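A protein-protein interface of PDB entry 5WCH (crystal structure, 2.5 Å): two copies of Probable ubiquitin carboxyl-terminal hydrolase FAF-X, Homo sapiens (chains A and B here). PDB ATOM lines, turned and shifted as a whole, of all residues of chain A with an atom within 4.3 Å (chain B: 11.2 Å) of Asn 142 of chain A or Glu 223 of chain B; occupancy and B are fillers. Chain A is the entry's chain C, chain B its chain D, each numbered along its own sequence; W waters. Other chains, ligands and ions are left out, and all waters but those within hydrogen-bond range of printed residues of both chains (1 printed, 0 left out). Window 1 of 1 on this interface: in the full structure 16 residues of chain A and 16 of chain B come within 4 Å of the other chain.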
ATOM      1  N   TRP A 125     -11.651  24.935 -10.357  1.00  0.00           N
ATOM      2  CA  TRP A 125     -12.480  23.959 -11.061  1.00  0.00           C
ATOM      3  C   TRP A 125     -13.061  24.516 -12.377  1.00  0.00           C
ATOM      4  O   TRP A 125     -14.285  24.484 -12.598  1.00  0.00           O
ATOM      5  CB  TRP A 125     -13.603  23.433 -10.158  1.00  0.00           C
ATOM      6  CG  TRP A 125     -13.213  23.112  -8.742  1.00  0.00           C
ATOM      7  CD1 TRP A 125     -13.923  23.433  -7.620  1.00  0.00           C
ATOM      8  CD2 TRP A 125     -12.039  22.418  -8.285  1.00  0.00           C
ATOM      9  NE1 TRP A 125     -13.274  22.988  -6.505  1.00  0.00           N
ATOM     10  CE2 TRP A 125     -12.115  22.360  -6.876  1.00  0.00           C
ATOM     11  CE3 TRP A 125     -10.926  21.848  -8.925  1.00  0.00           C
ATOM     12  CZ2 TRP A 125     -11.123  21.758  -6.094  1.00  0.00           C
ATOM     13  CZ3 TRP A 125      -9.940  21.250  -8.143  1.00  0.00           C
ATOM     14  CH2 TRP A 125     -10.049  21.211  -6.744  1.00  0.00           C
ATOM     15  N   LEU A 138      -9.435  24.959   1.860  1.00  0.00           N
ATOM     16  CA  LEU A 138      -8.973  23.618   1.476  1.00  0.00           C
ATOM     17  C   LEU A 138      -9.292  23.303   0.011  1.00  0.00           C
ATOM     18  O   LEU A 138      -8.497  22.691  -0.689  1.00  0.00           O
ATOM     19  CB  LEU A 138      -9.534  22.532   2.417  1.00  0.00           C
ATOM     20  CG  LEU A 138      -8.732  21.213   2.289  1.00  0.00           C
ATOM     21  CD1 LEU A 138      -7.402  21.251   3.033  1.00  0.00           C
ATOM     22  CD2 LEU A 138      -9.558  20.018   2.729  1.00  0.00           C
ATOM     23  N   GLU A 139     -10.451  23.736  -0.445  1.00  0.00           N
ATOM     24  CA  GLU A 139     -10.800  23.687  -1.857  1.00  0.00           C
ATOM     25  C   GLU A 139      -9.755  24.393  -2.726  1.00  0.00           C
ATOM     26  O   GLU A 139      -9.435  23.923  -3.815  1.00  0.00           O
ATOM     27  CB  GLU A 139     -12.156  24.337  -2.046  1.00  0.00           C
ATOM     28  CG  GLU A 139     -12.745  24.207  -3.425  1.00  0.00           C
ATOM     29  CD  GLU A 139     -14.231  24.579  -3.491  1.00  0.00           C
ATOM     30  OE1 GLU A 139     -14.907  24.673  -2.429  1.00  0.00           O
ATOM     31  OE2 GLU A 139     -14.719  24.774  -4.631  1.00  0.00           O
ATOM     32  N   PHE A 140      -9.230  25.516  -2.240  1.00  0.00           N
ATOM     33  CA  PHE A 140      -8.173  26.237  -2.939  1.00  0.00           C
ATOM     34  C   PHE A 140      -6.906  25.413  -2.968  1.00  0.00           C
ATOM     35  O   PHE A 140      -6.326  25.217  -4.029  1.00  0.00           O
ATOM     36  CB  PHE A 140      -7.885  27.606  -2.306  1.00  0.00           C
ATOM     37  CG  PHE A 140      -6.647  28.277  -2.857  1.00  0.00           C
ATOM     38  CD1 PHE A 140      -6.618  28.742  -4.167  1.00  0.00           C
ATOM     39  CD2 PHE A 140      -5.502  28.436  -2.070  1.00  0.00           C
ATOM     40  CE1 PHE A 140      -5.476  29.366  -4.678  1.00  0.00           C
ATOM     41  CE2 PHE A 140      -4.362  29.043  -2.577  1.00  0.00           C
ATOM     42  CZ  PHE A 140      -4.349  29.511  -3.878  1.00  0.00           C
ATOM     43  N   PHE A 141      -6.495  24.958  -1.786  1.00  0.00           N
ATOM     44  CA  PHE A 141      -5.305  24.128  -1.605  1.00  0.00           C
ATOM     45  C   PHE A 141      -5.290  22.902  -2.533  1.00  0.00           C
ATOM     46  O   PHE A 141      -4.274  22.623  -3.176  1.00  0.00           O
ATOM     47  CB  PHE A 141      -5.191  23.744  -0.124  1.00  0.00           C
ATOM     48  CG  PHE A 141      -4.166  22.679   0.194  1.00  0.00           C
ATOM     49  CD1 PHE A 141      -2.862  23.017   0.536  1.00  0.00           C
ATOM     50  CD2 PHE A 141      -4.537  21.331   0.244  1.00  0.00           C
ATOM     51  CE1 PHE A 141      -1.936  22.037   0.886  1.00  0.00           C
ATOM     52  CE2 PHE A 141      -3.618  20.341   0.586  1.00  0.00           C
ATOM     53  CZ  PHE A 141      -2.316  20.697   0.907  1.00  0.00           C
ATOM     54  N   ASN A 142      -6.404  22.183  -2.618  1.00  0.00           N
ATOM     55  CA  ASN A 142      -6.462  20.995  -3.481  1.00  0.00           C
ATOM     56  C   ASN A 142      -6.268  21.331  -4.939  1.00  0.00           C
ATOM     57  O   ASN A 142      -5.524  20.652  -5.649  1.00  0.00           O
ATOM     58  CB  ASN A 142      -7.774  20.236  -3.311  1.00  0.00           C
ATOM     59  CG  ASN A 142      -7.911  19.607  -1.938  1.00  0.00           C
ATOM     60  OD1 ASN A 142      -6.925  19.318  -1.270  1.00  0.00           O
ATOM     61  ND2 ASN A 142      -9.135  19.403  -1.512  1.00  0.00           N
ATOM     62  N   SER A 143      -6.920  22.392  -5.377  1.00  0.00           N
ATOM     63  CA  SER A 143      -6.796  22.831  -6.756  1.00  0.00           C
ATOM     64  C   SER A 143      -5.352  23.230  -7.097  1.00  0.00           C
ATOM     65  O   SER A 143      -4.830  22.867  -8.165  1.00  0.00           O
ATOM     66  CB  SER A 143      -7.739  23.988  -7.004  1.00  0.00           C
ATOM     67  OG  SER A 143      -7.956  24.170  -8.381  1.00  0.00           O
ATOM     68  N   LEU A 144      -4.715  23.942  -6.161  1.00  0.00           N
ATOM     69  CA  LEU A 144      -3.361  24.439  -6.323  1.00  0.00           C
ATOM     70  C   LEU A 144      -2.319  23.330  -6.312  1.00  0.00           C
ATOM     71  O   LEU A 144      -1.438  23.356  -7.167  1.00  0.00           O
ATOM     72  CB  LEU A 144      -3.017  25.479  -5.243  1.00  0.00           C
ATOM     73  CG  LEU A 144      -1.593  26.060  -5.273  1.00  0.00           C
ATOM     74  CD1 LEU A 144      -1.339  26.770  -6.594  1.00  0.00           C
ATOM     75  CD2 LEU A 144      -1.343  27.013  -4.125  1.00  0.00           C
ATOM     76  N   VAL A 145      -2.383  22.381  -5.365  1.00  0.00           N
ATOM     77  CA  VAL A 145      -1.405  21.273  -5.363  1.00  0.00           C
ATOM     78  C   VAL A 145      -1.592  20.393  -6.602  1.00  0.00           C
ATOM     79  O   VAL A 145      -0.610  20.026  -7.242  1.00  0.00           O
ATOM     80  CB  VAL A 145      -1.354  20.428  -4.058  1.00  0.00           C
ATOM     81  CG1 VAL A 145      -1.143  21.318  -2.835  1.00  0.00           C
ATOM     82  CG2 VAL A 145      -2.582  19.553  -3.884  1.00  0.00           C
ATOM     83  N   ASP A 146      -2.839  20.090  -6.962  1.00  0.00           N
ATOM     84  CA  ASP A 146      -3.100  19.345  -8.200  1.00  0.00           C
ATOM     85  C   ASP A 146      -2.428  20.022  -9.384  1.00  0.00           C
ATOM     86  O   ASP A 146      -1.690  19.375 -10.121  1.00  0.00           O
ATOM     87  CB  ASP A 146      -4.595  19.205  -8.477  1.00  0.00           C
ATOM     88  CG  ASP A 146      -5.294  18.208  -7.540  1.00  0.00           C
ATOM     89  OD1 ASP A 146      -4.685  17.745  -6.534  1.00  0.00           O
ATOM     90  OD2 ASP A 146      -6.487  17.913  -7.807  1.00  0.00           O
ATOM     91  N   SER A 187      -5.007   7.167  -1.584  1.00  0.00           N
ATOM     92  CA  SER A 187      -4.108   8.292  -1.333  1.00  0.00           C
ATOM     93  C   SER A 187      -4.872   9.430  -0.661  1.00  0.00           C
ATOM     94  O   SER A 187      -6.100   9.500  -0.752  1.00  0.00           O
ATOM     95  CB  SER A 187      -3.412   8.763  -2.611  1.00  0.00           C
ATOM     96  OG  SER A 187      -4.345   9.226  -3.564  1.00  0.00           O
ATOM     97  N   THR A 189      -4.272  13.844   0.435  1.00  0.00           N
ATOM     98  CA  THR A 189      -3.476  15.076   0.527  1.00  0.00           C
ATOM     99  C   THR A 189      -3.661  15.755   1.896  1.00  0.00           C
ATOM    100  O   THR A 189      -2.746  16.445   2.357  1.00  0.00           O
ATOM    101  CB  THR A 189      -3.790  16.043  -0.638  1.00  0.00           C
ATOM    102  OG1 THR A 189      -5.207  16.258  -0.720  1.00  0.00           O
ATOM    103  CG2 THR A 189      -3.301  15.450  -1.958  1.00  0.00           C
ATOM    104  N   LYS B 173     -18.023   7.324 -10.472  1.00  0.00           N
ATOM    105  CA  LYS B 173     -18.798   8.279  -9.685  1.00  0.00           C
ATOM    106  C   LYS B 173     -18.867   9.572 -10.466  1.00  0.00           C
ATOM    107  O   LYS B 173     -17.850  10.165 -10.752  1.00  0.00           O
ATOM    108  CB  LYS B 173     -18.158   8.497  -8.323  1.00  0.00           C
ATOM    109  CG  LYS B 173     -18.037   7.195  -7.541  1.00  0.00           C
ATOM    110  CD  LYS B 173     -17.813   7.420  -6.061  1.00  0.00           C
ATOM    111  CE  LYS B 173     -18.115   6.178  -5.228  1.00  0.00           C
ATOM    112  NZ  LYS B 173     -17.444   4.943  -5.730  1.00  0.00           N
ATOM    113  N   ILE B 174     -20.074   9.977 -10.844  1.00  0.00           N
ATOM    114  CA  ILE B 174     -20.282  11.180 -11.638  1.00  0.00           C
ATOM    115  C   ILE B 174     -20.999  12.206 -10.774  1.00  0.00           C
ATOM    116  O   ILE B 174     -22.199  12.075 -10.494  1.00  0.00           O
ATOM    117  CB  ILE B 174     -21.085  10.897 -12.932  1.00  0.00           C
ATOM    118  CG1 ILE B 174     -20.438   9.763 -13.735  1.00  0.00           C
ATOM    119  CG2 ILE B 174     -21.173  12.155 -13.796  1.00  0.00           C
ATOM    120  CD1 ILE B 174     -21.084   8.416 -13.506  1.00  0.00           C
ATOM    121  N   CYS B 175     -20.249  13.218 -10.341  1.00  0.00           N
ATOM    122  CA  CYS B 175     -20.774  14.266  -9.485  1.00  0.00           C
ATOM    123  C   CYS B 175     -21.690  15.194 -10.286  1.00  0.00           C
ATOM    124  O   CYS B 175     -21.336  15.627 -11.373  1.00  0.00           O
ATOM    125  CB  CYS B 175     -19.628  15.043  -8.841  1.00  0.00           C
ATOM    126  SG  CYS B 175     -18.593  14.037  -7.743  1.00  0.00           S
ATOM    127  N   GLY B 177     -23.367  17.978  -8.727  1.00  0.00           N
ATOM    128  CA  GLY B 177     -23.258  19.312  -8.135  1.00  0.00           C
ATOM    129  C   GLY B 177     -21.869  19.921  -8.204  1.00  0.00           C
ATOM    130  O   GLY B 177     -21.629  20.961  -7.590  1.00  0.00           O
ATOM    131  N   CYS B 178     -20.957  19.269  -8.930  1.00  0.00           N
ATOM    132  CA  CYS B 178     -19.586  19.763  -9.162  1.00  0.00           C
ATOM    133  C   CYS B 178     -19.055  19.045 -10.406  1.00  0.00           C
ATOM    134  O   CYS B 178     -19.675  18.084 -10.861  1.00  0.00           O
ATOM    135  CB  CYS B 178     -18.684  19.528  -7.927  1.00  0.00           C
ATOM    136  SG  CYS B 178     -17.929  17.883  -7.745  1.00  0.00           S
ATOM    137  N   PRO B 179     -17.917  19.506 -10.965  1.00  0.00           N
ATOM    138  CA  PRO B 179     -17.454  18.978 -12.240  1.00  0.00           C
ATOM    139  C   PRO B 179     -16.554  17.745 -12.161  1.00  0.00           C
ATOM    140  O   PRO B 179     -16.029  17.309 -13.190  1.00  0.00           O
ATOM    141  CB  PRO B 179     -16.670  20.159 -12.826  1.00  0.00           C
ATOM    142  CG  PRO B 179     -16.072  20.811 -11.627  1.00  0.00           C
ATOM    143  CD  PRO B 179     -17.040  20.593 -10.492  1.00  0.00           C
ATOM    144  N   HIS B 180     -16.381  17.167 -10.988  1.00  0.00           N
ATOM    145  CA  HIS B 180     -15.470  16.038 -10.857  1.00  0.00           C
ATOM    146  C   HIS B 180     -16.106  14.717 -11.256  1.00  0.00           C
ATOM    147  O   HIS B 180     -17.317  14.555 -11.206  1.00  0.00           O
ATOM    148  CB  HIS B 180     -14.931  15.952  -9.431  1.00  0.00           C
ATOM    149  CG  HIS B 180     -14.039  17.087  -9.079  1.00  0.00           C
ATOM    150  ND1 HIS B 180     -14.447  18.127  -8.278  1.00  0.00           N
ATOM    151  CD2 HIS B 180     -12.780  17.381  -9.472  1.00  0.00           C
ATOM    152  CE1 HIS B 180     -13.470  19.006  -8.169  1.00  0.00           C
ATOM    153  NE2 HIS B 180     -12.444  18.575  -8.884  1.00  0.00           N
ATOM    154  N   ARG B 181     -15.248  13.792 -11.658  1.00  0.00           N
ATOM    155  CA  ARG B 181     -15.587  12.395 -11.901  1.00  0.00           C
ATOM    156  C   ARG B 181     -14.435  11.541 -11.372  1.00  0.00           C
ATOM    157  O   ARG B 181     -13.267  11.919 -11.494  1.00  0.00           O
ATOM    158  CB  ARG B 181     -15.749  12.134 -13.398  1.00  0.00           C
ATOM    159  CG  ARG B 181     -17.157  12.296 -13.904  1.00  0.00           C
ATOM    160  CD  ARG B 181     -17.308  11.845 -15.355  1.00  0.00           C
ATOM    161  NE  ARG B 181     -17.042  10.411 -15.583  1.00  0.00           N
ATOM    162  CZ  ARG B 181     -17.453   9.722 -16.653  1.00  0.00           C
ATOM    163  NH1 ARG B 181     -18.166  10.295 -17.619  1.00  0.00           N
ATOM    164  NH2 ARG B 181     -17.162   8.432 -16.758  1.00  0.00           N
ATOM    165  N   TYR B 182     -14.768  10.400 -10.787  1.00  0.00           N
ATOM    166  CA  TYR B 182     -13.770   9.482 -10.268  1.00  0.00           C
ATOM    167  C   TYR B 182     -14.054   8.084 -10.810  1.00  0.00           C
ATOM    168  O   TYR B 182     -15.202   7.653 -10.835  1.00  0.00           O
ATOM    169  CB  TYR B 182     -13.797   9.474  -8.745  1.00  0.00           C
ATOM    170  CG  TYR B 182     -13.650  10.834  -8.085  1.00  0.00           C
ATOM    171  CD1 TYR B 182     -14.762  11.641  -7.855  1.00  0.00           C
ATOM    172  CD2 TYR B 182     -12.420  11.297  -7.656  1.00  0.00           C
ATOM    173  CE1 TYR B 182     -14.648  12.868  -7.236  1.00  0.00           C
ATOM    174  CE2 TYR B 182     -12.298  12.532  -7.028  1.00  0.00           C
ATOM    175  CZ  TYR B 182     -13.417  13.313  -6.824  1.00  0.00           C
ATOM    176  OH  TYR B 182     -13.314  14.541  -6.216  1.00  0.00           O
ATOM    177  N   GLU B 183     -13.019   7.389 -11.267  1.00  0.00           N
ATOM    178  CA  GLU B 183     -13.164   6.023 -11.754  1.00  0.00           C
ATOM    179  C   GLU B 183     -12.055   5.170 -11.187  1.00  0.00           C
ATOM    180  O   GLU B 183     -10.893   5.572 -11.261  1.00  0.00           O
ATOM    181  CB  GLU B 183     -13.099   5.970 -13.282  1.00  0.00           C
ATOM    182  CG  GLU B 183     -14.032   6.949 -13.990  1.00  0.00           C
ATOM    183  CD  GLU B 183     -14.158   6.718 -15.503  1.00  0.00           C
ATOM    184  OE1 GLU B 183     -13.828   5.606 -16.013  1.00  0.00           O
ATOM    185  OE2 GLU B 183     -14.610   7.669 -16.188  1.00  0.00           O
ATOM    186  N   CYS B 184     -12.406   4.011 -10.625  1.00  0.00           N
ATOM    187  CA  CYS B 184     -11.430   2.959 -10.334  1.00  0.00           C
ATOM    188  C   CYS B 184     -11.882   1.633 -10.928  1.00  0.00           C
ATOM    189  O   CYS B 184     -13.040   1.471 -11.296  1.00  0.00           O
ATOM    190  CB  CYS B 184     -11.171   2.821  -8.837  1.00  0.00           C
ATOM    191  SG  CYS B 184     -12.619   2.411  -7.856  1.00  0.00           S
ATOM    192  N   ALA B 219     -25.249  12.056   0.668  1.00  0.00           N
ATOM    193  CA  ALA B 219     -24.502  12.459  -0.525  1.00  0.00           C
ATOM    194  C   ALA B 219     -23.023  12.082  -0.455  1.00  0.00           C
ATOM    195  O   ALA B 219     -22.495  11.763   0.603  1.00  0.00           O
ATOM    196  CB  ALA B 219     -24.666  13.949  -0.801  1.00  0.00           C
ATOM    197  N   TYR B 220     -22.382  12.114  -1.616  1.00  0.00           N
ATOM    198  CA  TYR B 220     -21.000  11.712  -1.769  1.00  0.00           C
ATOM    199  C   TYR B 220     -20.048  12.854  -1.403  1.00  0.00           C
ATOM    200  O   TYR B 220     -20.260  14.000  -1.805  1.00  0.00           O
ATOM    201  CB  TYR B 220     -20.794  11.318  -3.224  1.00  0.00           C
ATOM    202  CG  TYR B 220     -19.391  10.920  -3.607  1.00  0.00           C
ATOM    203  CD1 TYR B 220     -18.834   9.732  -3.137  1.00  0.00           C
ATOM    204  CD2 TYR B 220     -18.638  11.706  -4.484  1.00  0.00           C
ATOM    205  CE1 TYR B 220     -17.551   9.355  -3.500  1.00  0.00           C
ATOM    206  CE2 TYR B 220     -17.355  11.334  -4.856  1.00  0.00           C
ATOM    207  CZ  TYR B 220     -16.814  10.156  -4.361  1.00  0.00           C
ATOM    208  OH  TYR B 220     -15.554   9.769  -4.739  1.00  0.00           O
ATOM    209  N   HIS B 221     -18.999  12.544  -0.646  1.00  0.00           N
ATOM    210  CA  HIS B 221     -17.968  13.540  -0.365  1.00  0.00           C
ATOM    211  C   HIS B 221     -17.014  13.652  -1.547  1.00  0.00           C
ATOM    212  O   HIS B 221     -16.276  12.721  -1.841  1.00  0.00           O
ATOM    213  CB  HIS B 221     -17.186  13.232   0.911  1.00  0.00           C
ATOM    214  CG  HIS B 221     -16.363  14.391   1.383  1.00  0.00           C
ATOM    215  ND1 HIS B 221     -15.085  14.631   0.923  1.00  0.00           N
ATOM    216  CD2 HIS B 221     -16.655  15.402   2.234  1.00  0.00           C
ATOM    217  CE1 HIS B 221     -14.615  15.727   1.492  1.00  0.00           C
ATOM    218  NE2 HIS B 221     -15.547  16.213   2.294  1.00  0.00           N
ATOM    219  N   CYS B 222     -17.064  14.782  -2.242  1.00  0.00           N
ATOM    220  CA  CYS B 222     -16.065  15.095  -3.273  1.00  0.00           C
ATOM    221  C   CYS B 222     -14.807  15.549  -2.544  1.00  0.00           C
ATOM    222  O   CYS B 222     -14.815  16.554  -1.840  1.00  0.00           O
ATOM    223  CB  CYS B 222     -16.511  16.201  -4.233  1.00  0.00           C
ATOM    224  SG  CYS B 222     -15.219  16.650  -5.430  1.00  0.00           S
ATOM    225  N   GLU B 223     -13.739  14.790  -2.723  1.00  0.00           N
ATOM    226  CA  GLU B 223     -12.488  14.997  -2.010  1.00  0.00           C
ATOM    227  C   GLU B 223     -11.824  16.304  -2.412  1.00  0.00           C
ATOM    228  O   GLU B 223     -11.140  16.916  -1.601  1.00  0.00           O
ATOM    229  CB  GLU B 223     -11.548  13.829  -2.317  1.00  0.00           C
ATOM    230  CG  GLU B 223     -10.346  13.660  -1.402  1.00  0.00           C
ATOM    231  CD  GLU B 223      -9.280  12.760  -2.023  1.00  0.00           C
ATOM    232  OE1 GLU B 223      -9.650  11.825  -2.783  1.00  0.00           O
ATOM    233  OE2 GLU B 223      -8.078  13.002  -1.761  1.00  0.00           O
ATOM    234  N   LYS B 224     -12.020  16.725  -3.663  1.00  0.00           N
ATOM    235  CA  LYS B 224     -11.384  17.935  -4.193  1.00  0.00           C
ATOM    236  C   LYS B 224     -12.144  19.162  -3.751  1.00  0.00           C
ATOM    237  O   LYS B 224     -11.564  20.095  -3.206  1.00  0.00           O
ATOM    238  CB  LYS B 224     -11.313  17.887  -5.730  1.00  0.00           C
ATOM    239  CG  LYS B 224     -10.550  16.703  -6.303  1.00  0.00           C
ATOM    240  CD  LYS B 224      -9.104  16.730  -5.855  1.00  0.00           C
ATOM    241  CE  LYS B 224      -8.270  15.640  -6.491  1.00  0.00           C
ATOM    242  NZ  LYS B 224      -6.940  15.560  -5.813  1.00  0.00           N
ATOM    243  N   CYS B 225     -13.449  19.158  -3.973  1.00  0.00           N
ATOM    244  CA  CYS B 225     -14.292  20.241  -3.512  1.00  0.00           C
ATOM    245  C   CYS B 225     -14.422  20.325  -1.987  1.00  0.00           C
ATOM    246  O   CYS B 225     -14.815  21.368  -1.470  1.00  0.00           O
ATOM    247  CB  CYS B 225     -15.679  20.125  -4.133  1.00  0.00           C
ATOM    248  SG  CYS B 225     -15.706  20.412  -5.916  1.00  0.00           S
ATOM    249  N   ASN B 226     -14.111  19.252  -1.264  1.00  0.00           N
ATOM    250  CA  ASN B 226     -14.265  19.238   0.203  1.00  0.00           C
ATOM    251  C   ASN B 226     -15.706  19.509   0.696  1.00  0.00           C
ATOM    252  O   ASN B 226     -15.923  20.328   1.564  1.00  0.00           O
ATOM    253  CB  ASN B 226     -13.262  20.205   0.872  1.00  0.00           C
ATOM    254  CG  ASN B 226     -13.140  19.970   2.368  1.00  0.00           C
ATOM    255  OD1 ASN B 226     -13.049  18.836   2.814  1.00  0.00           O
ATOM    256  ND2 ASN B 226     -13.158  21.036   3.142  1.00  0.00           N
ATOM    257  N   LYS B 227     -16.670  18.814   0.106  1.00  0.00           N
ATOM    258  CA  LYS B 227     -18.076  18.908   0.470  1.00  0.00           C
ATOM    259  C   LYS B 227     -18.864  17.714  -0.081  1.00  0.00           C
ATOM    260  O   LYS B 227     -18.362  16.954  -0.909  1.00  0.00           O
ATOM    261  CB  LYS B 227     -18.684  20.206  -0.059  1.00  0.00           C
ATOM    262  CG  LYS B 227     -18.889  20.228  -1.564  1.00  0.00           C
ATOM    263  CD  LYS B 227     -19.032  21.647  -2.100  1.00  0.00           C
ATOM    264  CE  LYS B 227     -19.733  21.648  -3.451  1.00  0.00           C
ATOM    265  NZ  LYS B 227     -19.266  22.744  -4.330  1.00  0.00           N
ATOM    266  N   LYS B 228     -20.096  17.567   0.397  1.00  0.00           N
ATOM    267  CA  LYS B 228     -21.037  16.572  -0.102  1.00  0.00           C
ATOM    268  C   LYS B 228     -21.671  17.103  -1.387  1.00  0.00           C
ATOM    269  O   LYS B 228     -22.084  18.266  -1.432  1.00  0.00           O
ATOM    270  CB  LYS B 228     -22.144  16.281   0.927  1.00  0.00           C
ATOM    271  CG  LYS B 228     -21.675  15.702   2.260  1.00  0.00           C
ATOM    272  CD  LYS B 228     -22.854  15.250   3.131  1.00  0.00           C
ATOM    273  N   VAL B 229     -21.726  16.261  -2.424  1.00  0.00           N
ATOM    274  CA  VAL B 229     -22.352  16.620  -3.704  1.00  0.00           C
ATOM    275  C   VAL B 229     -23.182  15.447  -4.207  1.00  0.00           C
ATOM    276  O   VAL B 229     -22.803  14.288  -3.989  1.00  0.00           O
ATOM    277  CB  VAL B 229     -21.326  17.028  -4.785  1.00  0.00           C
ATOM    278  CG1 VAL B 229     -20.478  18.197  -4.310  1.00  0.00           C
ATOM    279  CG2 VAL B 229     -20.439  15.863  -5.201  1.00  0.00           C
ATOM    280  N   ASP B 230     -24.304  15.747  -4.861  1.00  0.00           N
ATOM    281  CA  ASP B 230     -25.169  14.709  -5.415  1.00  0.00           C
ATOM    282  C   ASP B 230     -24.425  14.010  -6.532  1.00  0.00           C
ATOM    283  O   ASP B 230     -23.917  14.665  -7.448  1.00  0.00           O
ATOM    284  CB  ASP B 230     -26.495  15.281  -5.956  1.00  0.00           C
ATOM    285  CG  ASP B 230     -27.480  15.669  -4.847  1.00  0.00           C
ATOM    286  OD1 ASP B 230     -27.209  15.425  -3.645  1.00  0.00           O
ATOM    287  OD2 ASP B 230     -28.546  16.229  -5.185  1.00  0.00           O
ATOM    288  N   THR B 231     -24.374  12.683  -6.453  1.00  0.00           N
ATOM    289  CA  THR B 231     -23.528  11.884  -7.327  1.00  0.00           C
ATOM    290  C   THR B 231     -24.199  10.581  -7.768  1.00  0.00           C
ATOM    291  O   THR B 231     -24.844   9.903  -6.968  1.00  0.00           O
ATOM    292  CB  THR B 231     -22.208  11.570  -6.599  1.00  0.00           C
ATOM    293  OG1 THR B 231     -21.523  12.800  -6.323  1.00  0.00           O
ATOM    294  CG2 THR B 231     -21.299  10.654  -7.424  1.00  0.00           C
HETATM  295  O   HOH W   1      -6.895  14.374   0.310  1.00  0.00           O
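SG of Cys 225 of chain B sits close to NE1 of Trp 125 of chain A, at 3.6 Å. O of Glu 223 of chain B lies within hydrogen-bond range of ND2 of Asn 142 of chain A, 3.2 Å away. The side-chain amide nitrogen of Asn 142 of chain A is in hydrogen-bond range of the backbone carbonyl oxygen of Lys 224 of chain B (3.0 Å). NZ of Lys 224 of chain B is in salt-bridge range of OD2 of Asp 146 of chain A (3.1 Å). The side-chain carboxylate (OE1) of Glu 139 of chain A sits close to the backbone carbonyl oxygen (O) of Cys 225 of chain B.
NE1 of Trp 125 of chain A is in hydrogen-bond range of OE2 of Glu 139 of chain A (3.0 Å). The backbone carbonyl oxygen of Leu 138 of chain A lies close to the side-chain amide nitrogen of Asn 142 of chain A, 3.4 Å away. The backbone NH (N) of Cys 175 of chain B lies within hydrogen-bond range of the backbone carbonyl oxygen (O) of His 180 of chain B. SG of Cys 222 of chain B sits close to N of Lys 224 of chain B, 3.7 Å away.
Pro 179 of chain B touches Trp 125 of chain A. His 180 of chain B touches Trp 125 of chain A. Trp 125 of chain A touches Lys 224 of chain B (CZ2 to O, 3.4 Å). Leu 138 of chain A touches Asn 226 of chain B (CD2 to CG, 3.6 Å). Lys 224 of chain B touches Glu 139 of chain A (O to CA, 3.9 Å).
Of the printed residues of chain B, Trp 125 of chain A touches Pro 179 (3.9 Å), His 180 (3.6 Å), Lys 224 (3.4 Å) and Cys 225 (3.6 Å). Printed residues of chain B within 4 Å of Leu 138 of chain A: Asn 226. Of the printed residues of chain B, Glu 139 of chain A touches Lys 224 (3.9 Å) and Cys 225 (3.4 Å). Phe 140 of chain A touches none of the printed residues of chain B. No residue of chain B comes within 4 Å of Phe 141 of chain A. Printed residues of chain B within 4 Å of Asn 142 of chain A: Glu 223 (3.2 Å) and Lys 224 (3.0 Å). No residue of chain B comes within 4 Å of Val 145 of chain A. Of the printed residues of chain B, Asp 146 of chain A touches Lys 224. No residue of chain B comes within 4 Å of Ser 187 of chain A. No residue of chain B comes within 4 Å of Thr 189 of chain A. Of the printed residues of chain A, Pro 179 of chain B touches Trp 125. Of the printed residues of chain A, His 180 of chain B touches Trp 125. Glu 223 of chain B touches one residue of chain A. Of the printed residues of chain A, Cys 225 of chain B touches Trp 125 and Glu 139. The nearest residue of chain B that does not touch Asn 142 of chain A is Asn 226 of chain B (4.8 Å).
Of the 12 printed residues of chain A, 5 touch a printed residue of chain B. Hydrophobic or aromatic side chains of chain A that line the printed part of chain B: Trp 125 and Leu 138. Among the printed residues, Asp or Glu carboxylates within 4 Å of a Lys or Arg side-chain nitrogen of the other chain: Asp 146 of chain A with Lys 224 of chain B (3.1 Å).
No position is printed for both chains. Of the 10 pairs that touch across the chains among the printed residues, none has its exchanged pair printed and touching as well.
Water W1 bridges N of Thr 189 of chain A (2.7 Å) and OE2 of Glu 223 of chain B (2.8 Å).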
